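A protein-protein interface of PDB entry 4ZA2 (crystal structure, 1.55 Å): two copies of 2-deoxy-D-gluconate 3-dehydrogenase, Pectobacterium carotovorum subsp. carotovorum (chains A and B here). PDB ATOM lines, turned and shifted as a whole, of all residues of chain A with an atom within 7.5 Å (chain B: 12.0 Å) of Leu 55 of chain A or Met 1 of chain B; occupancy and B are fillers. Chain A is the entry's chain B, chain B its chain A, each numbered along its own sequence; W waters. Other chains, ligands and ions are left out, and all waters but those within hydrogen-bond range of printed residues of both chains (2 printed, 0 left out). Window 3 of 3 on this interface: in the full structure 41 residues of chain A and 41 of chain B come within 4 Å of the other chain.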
ATOM      1  N   ALA A  27       6.761  13.306  -9.347  1.00  0.00           N
ATOM      2  CA  ALA A  27       5.500  12.599  -9.505  1.00  0.00           C
ATOM      3  C   ALA A  27       4.596  13.204 -10.573  1.00  0.00           C
ATOM      4  O   ALA A  27       4.004  12.473 -11.357  1.00  0.00           O
ATOM      5  CB  ALA A  27       4.743  12.545  -8.188  1.00  0.00           C
ATOM      6  N   ILE A  28       4.482  14.533 -10.594  1.00  0.00           N
ATOM      7  CA  ILE A  28       3.677  15.199 -11.605  1.00  0.00           C
ATOM      8  C   ILE A  28       4.245  14.966 -13.012  1.00  0.00           C
ATOM      9  O   ILE A  28       3.496  14.663 -13.940  1.00  0.00           O
ATOM     10  CB  ILE A  28       3.495  16.706 -11.305  1.00  0.00           C
ATOM     11  CG1 ILE A  28       2.582  16.871 -10.077  1.00  0.00           C
ATOM     12  CG2 ILE A  28       2.897  17.429 -12.496  1.00  0.00           C
ATOM     13  CD1 ILE A  28       2.644  18.250  -9.445  1.00  0.00           C
ATOM     14  N   GLY A  29       5.562  15.072 -13.154  1.00  0.00           N
ATOM     15  CA  GLY A  29       6.195  14.859 -14.455  1.00  0.00           C
ATOM     16  C   GLY A  29       5.955  13.446 -14.967  1.00  0.00           C
ATOM     17  O   GLY A  29       5.563  13.230 -16.106  1.00  0.00           O
ATOM     18  N   LEU A  30       6.135  12.463 -14.092  1.00  0.00           N
ATOM     19  CA  LEU A  30       5.866  11.094 -14.450  1.00  0.00           C
ATOM     20  C   LEU A  30       4.395  10.903 -14.854  1.00  0.00           C
ATOM     21  O   LEU A  30       4.106  10.236 -15.849  1.00  0.00           O
ATOM     22  CB  LEU A  30       6.287  10.142 -13.318  1.00  0.00           C
ATOM     23  CG  LEU A  30       7.803  10.082 -13.136  1.00  0.00           C
ATOM     24  CD1 LEU A  30       8.181   9.476 -11.801  1.00  0.00           C
ATOM     25  CD2 LEU A  30       8.445   9.296 -14.262  1.00  0.00           C
ATOM     26  N   ALA A  31       3.478  11.525 -14.107  1.00  0.00           N
ATOM     27  CA  ALA A  31       2.052  11.459 -14.431  1.00  0.00           C
ATOM     28  C   ALA A  31       1.747  12.090 -15.788  1.00  0.00           C
ATOM     29  O   ALA A  31       0.963  11.555 -16.570  1.00  0.00           O
ATOM     30  CB  ALA A  31       1.234  12.144 -13.333  1.00  0.00           C
ATOM     31  N   GLN A  32       2.371  13.225 -16.051  1.00  0.00           N
ATOM     32  CA  GLN A  32       2.225  13.917 -17.328  1.00  0.00           C
ATOM     33  C   GLN A  32       2.659  13.029 -18.503  1.00  0.00           C
ATOM     34  O   GLN A  32       2.071  13.064 -19.594  1.00  0.00           O
ATOM     35  CB  GLN A  32       3.015  15.226 -17.323  1.00  0.00           C
ATOM     36  CG  GLN A  32       2.373  16.344 -16.500  1.00  0.00           C
ATOM     37  CD  GLN A  32       3.128  17.665 -16.586  1.00  0.00           C
ATOM     38  OE1 GLN A  32       4.073  17.813 -17.363  1.00  0.00           O
ATOM     39  NE2 GLN A  32       2.704  18.642 -15.782  1.00  0.00           N
ATOM     40  N   ALA A  33       3.708  12.245 -18.284  1.00  0.00           N
ATOM     41  CA  ALA A  33       4.205  11.312 -19.284  1.00  0.00           C
ATOM     42  C   ALA A  33       3.366  10.034 -19.425  1.00  0.00           C
ATOM     43  O   ALA A  33       3.621   9.208 -20.311  1.00  0.00           O
ATOM     44  CB  ALA A  33       5.659  10.960 -18.966  1.00  0.00           C
ATOM     45  N   GLY A  34       2.383   9.838 -18.535  1.00  0.00           N
ATOM     46  CA  GLY A  34       1.463   8.710 -18.643  1.00  0.00           C
ATOM     47  C   GLY A  34       1.374   7.763 -17.459  1.00  0.00           C
ATOM     48  O   GLY A  34       0.533   6.857 -17.452  1.00  0.00           O
ATOM     49  N   CYS A  35       2.234   7.954 -16.466  1.00  0.00           N
ATOM     50  CA  CYS A  35       2.294   7.050 -15.329  1.00  0.00           C
ATOM     51  C   CYS A  35       1.120   7.226 -14.399  1.00  0.00           C
ATOM     52  O   CYS A  35       0.779   8.344 -14.055  1.00  0.00           O
ATOM     53  CB  CYS A  35       3.510   7.315 -14.471  1.00  0.00           C
ATOM     54  SG  CYS A  35       5.047   6.763 -15.210  1.00  0.00           S
ATOM     55  N   THR A  48      -0.490  17.188  -4.518  1.00  0.00           N
ATOM     56  CA  THR A  48       0.013  16.274  -5.542  1.00  0.00           C
ATOM     57  C   THR A  48      -1.095  15.377  -6.108  1.00  0.00           C
ATOM     58  O   THR A  48      -1.209  15.232  -7.319  1.00  0.00           O
ATOM     59  CB  THR A  48       1.185  15.434  -4.989  1.00  0.00           C
ATOM     60  OG1 THR A  48       2.169  16.298  -4.420  1.00  0.00           O
ATOM     61  CG2 THR A  48       1.828  14.585  -6.098  1.00  0.00           C
ATOM     62  N   ILE A  49      -1.935  14.804  -5.237  1.00  0.00           N
ATOM     63  CA  ILE A  49      -3.043  13.965  -5.679  1.00  0.00           C
ATOM     64  C   ILE A  49      -3.999  14.742  -6.597  1.00  0.00           C
ATOM     65  O   ILE A  49      -4.437  14.232  -7.618  1.00  0.00           O
ATOM     66  CB  ILE A  49      -3.808  13.376  -4.472  1.00  0.00           C
ATOM     67  CG1 ILE A  49      -2.898  12.404  -3.705  1.00  0.00           C
ATOM     68  CG2 ILE A  49      -5.076  12.660  -4.931  1.00  0.00           C
ATOM     69  CD1 ILE A  49      -3.364  12.054  -2.302  1.00  0.00           C
ATOM     70  N   GLU A  50      -4.343  15.960  -6.199  1.00  0.00           N
ATOM     71  CA  GLU A  50      -5.216  16.810  -7.018  1.00  0.00           C
ATOM     72  C   GLU A  50      -4.652  16.999  -8.426  1.00  0.00           C
ATOM     73  O   GLU A  50      -5.362  16.852  -9.415  1.00  0.00           O
ATOM     74  CB  GLU A  50      -5.435  18.167  -6.346  1.00  0.00           C
ATOM     75  CG  GLU A  50      -6.354  18.096  -5.128  1.00  0.00           C
ATOM     76  CD  GLU A  50      -6.508  19.429  -4.402  1.00  0.00           C
ATOM     77  OE1 GLU A  50      -6.100  20.474  -4.974  1.00  0.00           O
ATOM     78  OE2 GLU A  50      -7.048  19.431  -3.259  1.00  0.00           O
ATOM     79  N   LYS A  51      -3.355  17.275  -8.503  1.00  0.00           N
ATOM     80  CA  LYS A  51      -2.710  17.540  -9.783  1.00  0.00           C
ATOM     81  C   LYS A  51      -2.580  16.291 -10.639  1.00  0.00           C
ATOM     82  O   LYS A  51      -2.820  16.326 -11.842  1.00  0.00           O
ATOM     83  CB  LYS A  51      -1.363  18.215  -9.548  1.00  0.00           C
ATOM     84  CG  LYS A  51      -1.526  19.672  -9.141  1.00  0.00           C
ATOM     85  CD  LYS A  51      -0.328  20.235  -8.408  1.00  0.00           C
ATOM     86  CE  LYS A  51      -0.504  21.731  -8.193  1.00  0.00           C
ATOM     87  NZ  LYS A  51       0.597  22.321  -7.386  1.00  0.00           N
ATOM     88  N   VAL A  52      -2.251  15.167 -10.014  1.00  0.00           N
ATOM     89  CA  VAL A  52      -2.122  13.923 -10.742  1.00  0.00           C
ATOM     90  C   VAL A  52      -3.479  13.492 -11.284  1.00  0.00           C
ATOM     91  O   VAL A  52      -3.605  13.152 -12.450  1.00  0.00           O
ATOM     92  CB  VAL A  52      -1.473  12.820  -9.868  1.00  0.00           C
ATOM     93  CG1 VAL A  52      -1.555  11.459 -10.539  1.00  0.00           C
ATOM     94  CG2 VAL A  52      -0.027  13.180  -9.598  1.00  0.00           C
ATOM     95  N   THR A  53      -4.504  13.541 -10.437  1.00  0.00           N
ATOM     96  CA  THR A  53      -5.828  13.085 -10.835  1.00  0.00           C
ATOM     97  C   THR A  53      -6.459  14.017 -11.883  1.00  0.00           C
ATOM     98  O   THR A  53      -7.224  13.576 -12.747  1.00  0.00           O
ATOM     99  CB  THR A  53      -6.729  12.883  -9.598  1.00  0.00           C
ATOM    100  OG1 THR A  53      -6.751  14.072  -8.811  1.00  0.00           O
ATOM    101  CG2 THR A  53      -6.182  11.747  -8.744  1.00  0.00           C
ATOM    102  N   ALA A  54      -6.079  15.291 -11.842  1.00  0.00           N
ATOM    103  CA  ALA A  54      -6.508  16.255 -12.864  1.00  0.00           C
ATOM    104  C   ALA A  54      -5.967  15.895 -14.254  1.00  0.00           C
ATOM    105  O   ALA A  54      -6.603  16.191 -15.257  1.00  0.00           O
ATOM    106  CB  ALA A  54      -6.098  17.665 -12.481  1.00  0.00           C
ATOM    107  N   LEU A  55      -4.809  15.239 -14.308  1.00  0.00           N
ATOM    108  CA  LEU A  55      -4.271  14.742 -15.584  1.00  0.00           C
ATOM    109  C   LEU A  55      -4.995  13.503 -16.117  1.00  0.00           C
ATOM    110  O   LEU A  55      -4.707  13.041 -17.234  1.00  0.00           O
ATOM    111  CB  LEU A  55      -2.776  14.431 -15.426  1.00  0.00           C
ATOM    112  CG  LEU A  55      -1.899  15.640 -15.105  1.00  0.00           C
ATOM    113  CD1 LEU A  55      -0.561  15.217 -14.525  1.00  0.00           C
ATOM    114  CD2 LEU A  55      -1.685  16.470 -16.364  1.00  0.00           C
ATOM    115  N   GLY A  56      -5.929  12.954 -15.334  1.00  0.00           N
ATOM    116  CA  GLY A  56      -6.634  11.735 -15.709  1.00  0.00           C
ATOM    117  C   GLY A  56      -5.922  10.476 -15.268  1.00  0.00           C
ATOM    118  O   GLY A  56      -6.291   9.383 -15.684  1.00  0.00           O
ATOM    119  N   ARG A  57      -4.919  10.635 -14.412  1.00  0.00           N
ATOM    120  CA  ARG A  57      -4.119   9.516 -13.922  1.00  0.00           C
ATOM    121  C   ARG A  57      -4.597   9.072 -12.543  1.00  0.00           C
ATOM    122  O   ARG A  57      -5.225   9.849 -11.814  1.00  0.00           O
ATOM    123  CB  ARG A  57      -2.640   9.914 -13.849  1.00  0.00           C
ATOM    124  CG  ARG A  57      -2.033  10.360 -15.176  1.00  0.00           C
ATOM    125  CD  ARG A  57      -1.501   9.202 -15.994  1.00  0.00           C
ATOM    126  NE  ARG A  57      -2.547   8.297 -16.462  1.00  0.00           N
ATOM    127  CZ  ARG A  57      -3.301   8.493 -17.543  1.00  0.00           C
ATOM    128  NH1 ARG A  57      -3.151   9.576 -18.302  1.00  0.00           N
ATOM    129  NH2 ARG A  57      -4.220   7.588 -17.867  1.00  0.00           N
ATOM    130  N   ARG A  58      -4.309   7.822 -12.200  1.00  0.00           N
ATOM    131  CA  ARG A  58      -4.620   7.281 -10.882  1.00  0.00           C
ATOM    132  C   ARG A  58      -3.512   7.606  -9.892  1.00  0.00           C
ATOM    133  O   ARG A  58      -2.332   7.678 -10.258  1.00  0.00           O
ATOM    134  CB  ARG A  58      -4.775   5.763 -10.948  1.00  0.00           C
ATOM    135  CG  ARG A  58      -6.124   5.254 -11.434  1.00  0.00           C
ATOM    136  CD  ARG A  58      -6.407   3.858 -10.868  1.00  0.00           C
ATOM    137  NE  ARG A  58      -5.927   2.796 -11.743  1.00  0.00           N
ATOM    138  CZ  ARG A  58      -5.762   1.515 -11.413  1.00  0.00           C
ATOM    139  NH1 ARG A  58      -6.013   1.059 -10.178  1.00  0.00           N
ATOM    140  NH2 ARG A  58      -5.317   0.675 -12.346  1.00  0.00           N
ATOM    141  N   MET A 225      11.470  17.117 -13.940  1.00  0.00           N
ATOM    142  CA  MET A 225      10.454  16.360 -14.648  1.00  0.00           C
ATOM    143  C   MET A 225      11.039  15.629 -15.856  1.00  0.00           C
ATOM    144  O   MET A 225      10.872  14.417 -16.009  1.00  0.00           O
ATOM    145  CB  MET A 225       9.300  17.275 -15.056  1.00  0.00           C
ATOM    146  CG  MET A 225       8.528  17.756 -13.851  1.00  0.00           C
ATOM    147  SD  MET A 225       7.151  18.740 -14.409  1.00  0.00           S
ATOM    148  CE  MET A 225       6.383  19.144 -12.829  1.00  0.00           C
ATOM    149  N   MET B   1       2.940  20.151 -20.103  1.00  0.00           N
ATOM    150  CA  MET B   1       2.921  18.677 -20.330  1.00  0.00           C
ATOM    151  C   MET B   1       4.294  18.197 -20.807  1.00  0.00           C
ATOM    152  O   MET B   1       4.737  18.534 -21.907  1.00  0.00           O
ATOM    153  CB  MET B   1       1.822  18.305 -21.323  1.00  0.00           C
ATOM    154  CG  MET B   1       0.415  18.607 -20.820  1.00  0.00           C
ATOM    155  SD  MET B   1      -0.073  17.608 -19.391  1.00  0.00           S
ATOM    156  CE  MET B   1      -0.193  15.986 -20.120  1.00  0.00           C
ATOM    157  N   ILE B   2       4.945  17.399 -19.961  1.00  0.00           N
ATOM    158  CA  ILE B   2       6.372  17.086 -20.099  1.00  0.00           C
ATOM    159  C   ILE B   2       6.781  16.411 -21.404  1.00  0.00           C
ATOM    160  O   ILE B   2       7.898  16.606 -21.864  1.00  0.00           O
ATOM    161  CB  ILE B   2       6.876  16.227 -18.918  1.00  0.00           C
ATOM    162  CG1 ILE B   2       8.411  16.214 -18.869  1.00  0.00           C
ATOM    163  CG2 ILE B   2       6.335  14.809 -18.986  1.00  0.00           C
ATOM    164  CD1 ILE B   2       9.038  17.591 -18.743  1.00  0.00           C
ATOM    165  N   LEU B   3       5.909  15.613 -22.006  1.00  0.00           N
ATOM    166  CA  LEU B   3       6.304  14.954 -23.241  1.00  0.00           C
ATOM    167  C   LEU B   3       6.557  15.980 -24.334  1.00  0.00           C
ATOM    168  O   LEU B   3       7.383  15.729 -25.198  1.00  0.00           O
ATOM    169  CB  LEU B   3       5.326  13.875 -23.691  1.00  0.00           C
ATOM    170  CG  LEU B   3       5.227  12.669 -22.746  1.00  0.00           C
ATOM    171  CD1 LEU B   3       4.096  11.751 -23.192  1.00  0.00           C
ATOM    172  CD2 LEU B   3       6.544  11.893 -22.620  1.00  0.00           C
ATOM    173  N   ASN B   4       5.905  17.146 -24.272  1.00  0.00           N
ATOM    174  CA  ASN B   4       6.180  18.222 -25.232  1.00  0.00           C
ATOM    175  C   ASN B   4       7.619  18.727 -25.135  1.00  0.00           C
ATOM    176  O   ASN B   4       8.173  19.205 -26.131  1.00  0.00           O
ATOM    177  CB  ASN B   4       5.223  19.405 -25.041  1.00  0.00           C
ATOM    178  CG  ASN B   4       3.789  19.068 -25.395  1.00  0.00           C
ATOM    179  OD1 ASN B   4       3.520  18.240 -26.271  1.00  0.00           O
ATOM    180  ND2 ASN B   4       2.852  19.740 -24.736  1.00  0.00           N
ATOM    181  N   SER B   5       8.224  18.604 -23.953  1.00  0.00           N
ATOM    182  CA  SER B   5       9.591  19.079 -23.732  1.00  0.00           C
ATOM    183  C   SER B   5      10.628  18.284 -24.505  1.00  0.00           C
ATOM    184  O   SER B   5      11.727  18.775 -24.708  1.00  0.00           O
ATOM    185  CB  SER B   5       9.944  19.052 -22.251  1.00  0.00           C
ATOM    186  OG  SER B   5       9.068  19.898 -21.533  1.00  0.00           O
ATOM    187  N   PHE B   6      10.288  17.069 -24.922  1.00  0.00           N
ATOM    188  CA  PHE B   6      11.211  16.238 -25.696  1.00  0.00           C
ATOM    189  C   PHE B   6      11.073  16.452 -27.200  1.00  0.00           C
ATOM    190  O   PHE B   6      11.919  16.000 -27.963  1.00  0.00           O
ATOM    191  CB  PHE B   6      10.989  14.752 -25.416  1.00  0.00           C
ATOM    192  CG  PHE B   6      11.224  14.353 -23.987  1.00  0.00           C
ATOM    193  CD1 PHE B   6      12.500  14.209 -23.487  1.00  0.00           C
ATOM    194  CD2 PHE B   6      10.160  14.086 -23.155  1.00  0.00           C
ATOM    195  CE1 PHE B   6      12.706  13.822 -22.173  1.00  0.00           C
ATOM    196  CE2 PHE B   6      10.363  13.716 -21.839  1.00  0.00           C
ATOM    197  CZ  PHE B   6      11.634  13.583 -21.346  1.00  0.00           C
ATOM    198  N   ASP B   7       9.984  17.097 -27.615  1.00  0.00           N
ATOM    199  CA  ASP B   7       9.647  17.288 -29.022  1.00  0.00           C
ATOM    200  C   ASP B   7      10.542  18.351 -29.640  1.00  0.00           C
ATOM    201  O   ASP B   7      10.559  19.484 -29.170  1.00  0.00           O
ATOM    202  CB  ASP B   7       8.167  17.718 -29.113  1.00  0.00           C
ATOM    203  CG  ASP B   7       7.616  17.693 -30.525  1.00  0.00           C
ATOM    204  OD1 ASP B   7       8.388  17.686 -31.498  1.00  0.00           O
ATOM    205  OD2 ASP B   7       6.371  17.732 -30.655  1.00  0.00           O
ATOM    206  N   LEU B   8      11.262  17.990 -30.703  1.00  0.00           N
ATOM    207  CA  LEU B   8      12.196  18.894 -31.371  1.00  0.00           C
ATOM    208  C   LEU B   8      11.639  19.385 -32.713  1.00  0.00           C
ATOM    209  O   LEU B   8      12.397  19.794 -33.589  1.00  0.00           O
ATOM    210  CB  LEU B   8      13.560  18.207 -31.560  1.00  0.00           C
ATOM    211  CG  LEU B   8      14.195  17.633 -30.290  1.00  0.00           C
ATOM    212  CD1 LEU B   8      15.528  16.962 -30.581  1.00  0.00           C
ATOM    213  CD2 LEU B   8      14.349  18.736 -29.261  1.00  0.00           C
ATOM    214  N   GLN B   9      10.312  19.398 -32.852  1.00  0.00           N
ATOM    215  CA  GLN B   9       9.680  19.972 -34.024  1.00  0.00           C
ATOM    216  C   GLN B   9      10.206  21.394 -34.225  1.00  0.00           C
ATOM    217  O   GLN B   9      10.291  22.179 -33.286  1.00  0.00           O
ATOM    218  CB  GLN B   9       8.151  19.992 -33.855  1.00  0.00           C
ATOM    219  CG  GLN B   9       7.395  20.610 -35.025  1.00  0.00           C
ATOM    220  CD  GLN B   9       5.921  20.857 -34.724  1.00  0.00           C
ATOM    221  OE1 GLN B   9       5.533  21.101 -33.575  1.00  0.00           O
ATOM    222  NE2 GLN B   9       5.088  20.799 -35.762  1.00  0.00           N
ATOM    223  N   SER B 233      17.039  18.780 -26.034  1.00  0.00           N
ATOM    224  CA  SER B 233      15.674  19.252 -25.784  1.00  0.00           C
ATOM    225  C   SER B 233      15.531  20.088 -24.517  1.00  0.00           C
ATOM    226  O   SER B 233      16.411  20.129 -23.667  1.00  0.00           O
ATOM    227  CB  SER B 233      14.722  18.066 -25.686  1.00  0.00           C
ATOM    228  OG  SER B 233      14.827  17.423 -24.418  1.00  0.00           O
ATOM    229  N   SER B 234      14.385  20.757 -24.396  1.00  0.00           N
ATOM    230  CA  SER B 234      14.092  21.530 -23.192  1.00  0.00           C
ATOM    231  C   SER B 234      13.927  20.657 -21.948  1.00  0.00           C
ATOM    232  O   SER B 234      14.011  21.166 -20.841  1.00  0.00           O
ATOM    233  CB  SER B 234      12.843  22.402 -23.392  1.00  0.00           C
ATOM    234  OG  SER B 234      11.708  21.606 -23.587  1.00  0.00           O
ATOM    235  N   ALA B 235      13.738  19.350 -22.130  1.00  0.00           N
ATOM    236  CA  ALA B 235      13.657  18.418 -20.990  1.00  0.00           C
ATOM    237  C   ALA B 235      14.926  18.345 -20.134  1.00  0.00           C
ATOM    238  O   ALA B 235      14.908  17.780 -19.032  1.00  0.00           O
ATOM    239  CB  ALA B 235      13.291  17.032 -21.499  1.00  0.00           C
ATOM    240  N   SER B 236      16.040  18.876 -20.640  1.00  0.00           N
ATOM    241  CA  SER B 236      17.314  18.847 -19.935  1.00  0.00           C
ATOM    242  C   SER B 236      17.896  20.241 -19.673  1.00  0.00           C
ATOM    243  O   SER B 236      19.108  20.407 -19.531  1.00  0.00           O
ATOM    244  CB  SER B 236      18.312  17.990 -20.710  1.00  0.00           C
ATOM    245  OG  SER B 236      18.573  18.525 -21.989  1.00  0.00           O
ATOM    246  N   ASP B 237      17.025  21.241 -19.567  1.00  0.00           N
ATOM    247  CA  ASP B 237      17.461  22.620 -19.490  1.00  0.00           C
ATOM    248  C   ASP B 237      18.338  22.974 -18.288  1.00  0.00           C
ATOM    249  O   ASP B 237      19.166  23.872 -18.396  1.00  0.00           O
ATOM    250  CB  ASP B 237      16.253  23.575 -19.535  1.00  0.00           C
ATOM    251  CG  ASP B 237      15.762  23.853 -20.957  1.00  0.00           C
ATOM    252  OD1 ASP B 237      16.410  23.464 -21.956  1.00  0.00           O
ATOM    253  OD2 ASP B 237      14.680  24.475 -21.082  1.00  0.00           O
HETATM  254  O   HOH W   1       3.057  15.002 -21.467  1.00  0.00           O
HETATM  255  O   HOH W   2       5.486  19.956 -18.106  1.00  0.00           O
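The backbone NH (N) of Ile 2 of chain B sits at hydrogen-bond distance from the side-chain amide oxygen (OE1) of Gln 32 of chain A, 2.8 Å away.
Among the printed residues, merely in contact across the chains: Gln 32 of chain A with Met 1 of chain B (3.3 Å), Gly 29 of chain A with Ile 2 of chain B (3.4 Å), Leu 55 of chain A with Met 1 of chain B (3.6 Å), Met 225 of chain A with Ile 2 of chain B (3.7 Å), Ala 33 of chain A with Ile 2 of chain B (3.7 Å) and Ala 33 of chain A with Leu 3 of chain B (3.9 Å).
No residue of chain B comes within 4 Å of Ile 28 of chain A.
Of chain B, only Ile 2 comes within 4 Å of Gly 29 of chain A.
No residue of chain B comes within 4 Å of Ala 31 of chain A.
Gln 32 of chain A touches two residues of chain B.
No residue of chain B comes within 4 Å of Gly 56 of chain A.
Arg 57 of chain A touches none of the printed residues of chain B.
Of the printed residues of chain B, Met 225 of chain A touches Ile 2 (3.7 Å).
Met 1 of chain B touches two residues of chain A.
Printed residues of chain A within 4 Å of Ile 2 of chain B: Gly 29, Gln 32, Ala 33 and Met 225.
Of the printed residues of chain A, Leu 3 of chain B touches Ala 33 (3.9 Å).
The nearest residue of chain A that does not touch Met 1 of chain B is Ala 33 of chain A (5.7 Å).
The nearest printed residue of chain B that does not touch Met 225 of chain A is Ala 235 of chain B (5.4 Å).
Hydrophobic or aromatic side chains of chain A within 4 Å of the printed part of chain B: Ala 33, Leu 55 and Met 225.
Of the 14 printed residues of chain B, 3 touch a printed residue of chain A.
Among the printed residues, no Asp or Glu carboxylate lies within 4 Å of a Lys or Arg side-chain nitrogen of the other chain.
No position is printed for both chains.
Of the 7 pairs that touch across the chains among the printed residues, none has its exchanged pair printed and touching as well.
Water W2 lies within hydrogen-bond range of the side-chain amide oxygen (OE1) of Gln 32 of chain A, the backbone NH (N) of Ile 2 of chain B and the backbone NH (N) of Met 1 of chain B.
Water W1 lies within hydrogen-bond range of the backbone carbonyl oxygen (O) of Gln 32 of chain A (2.9 Å), the backbone NH (N) of Leu 3 of chain B (3.0 Å) and the backbone NH (N) of Ile 2 of chain B (3.4 Å).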
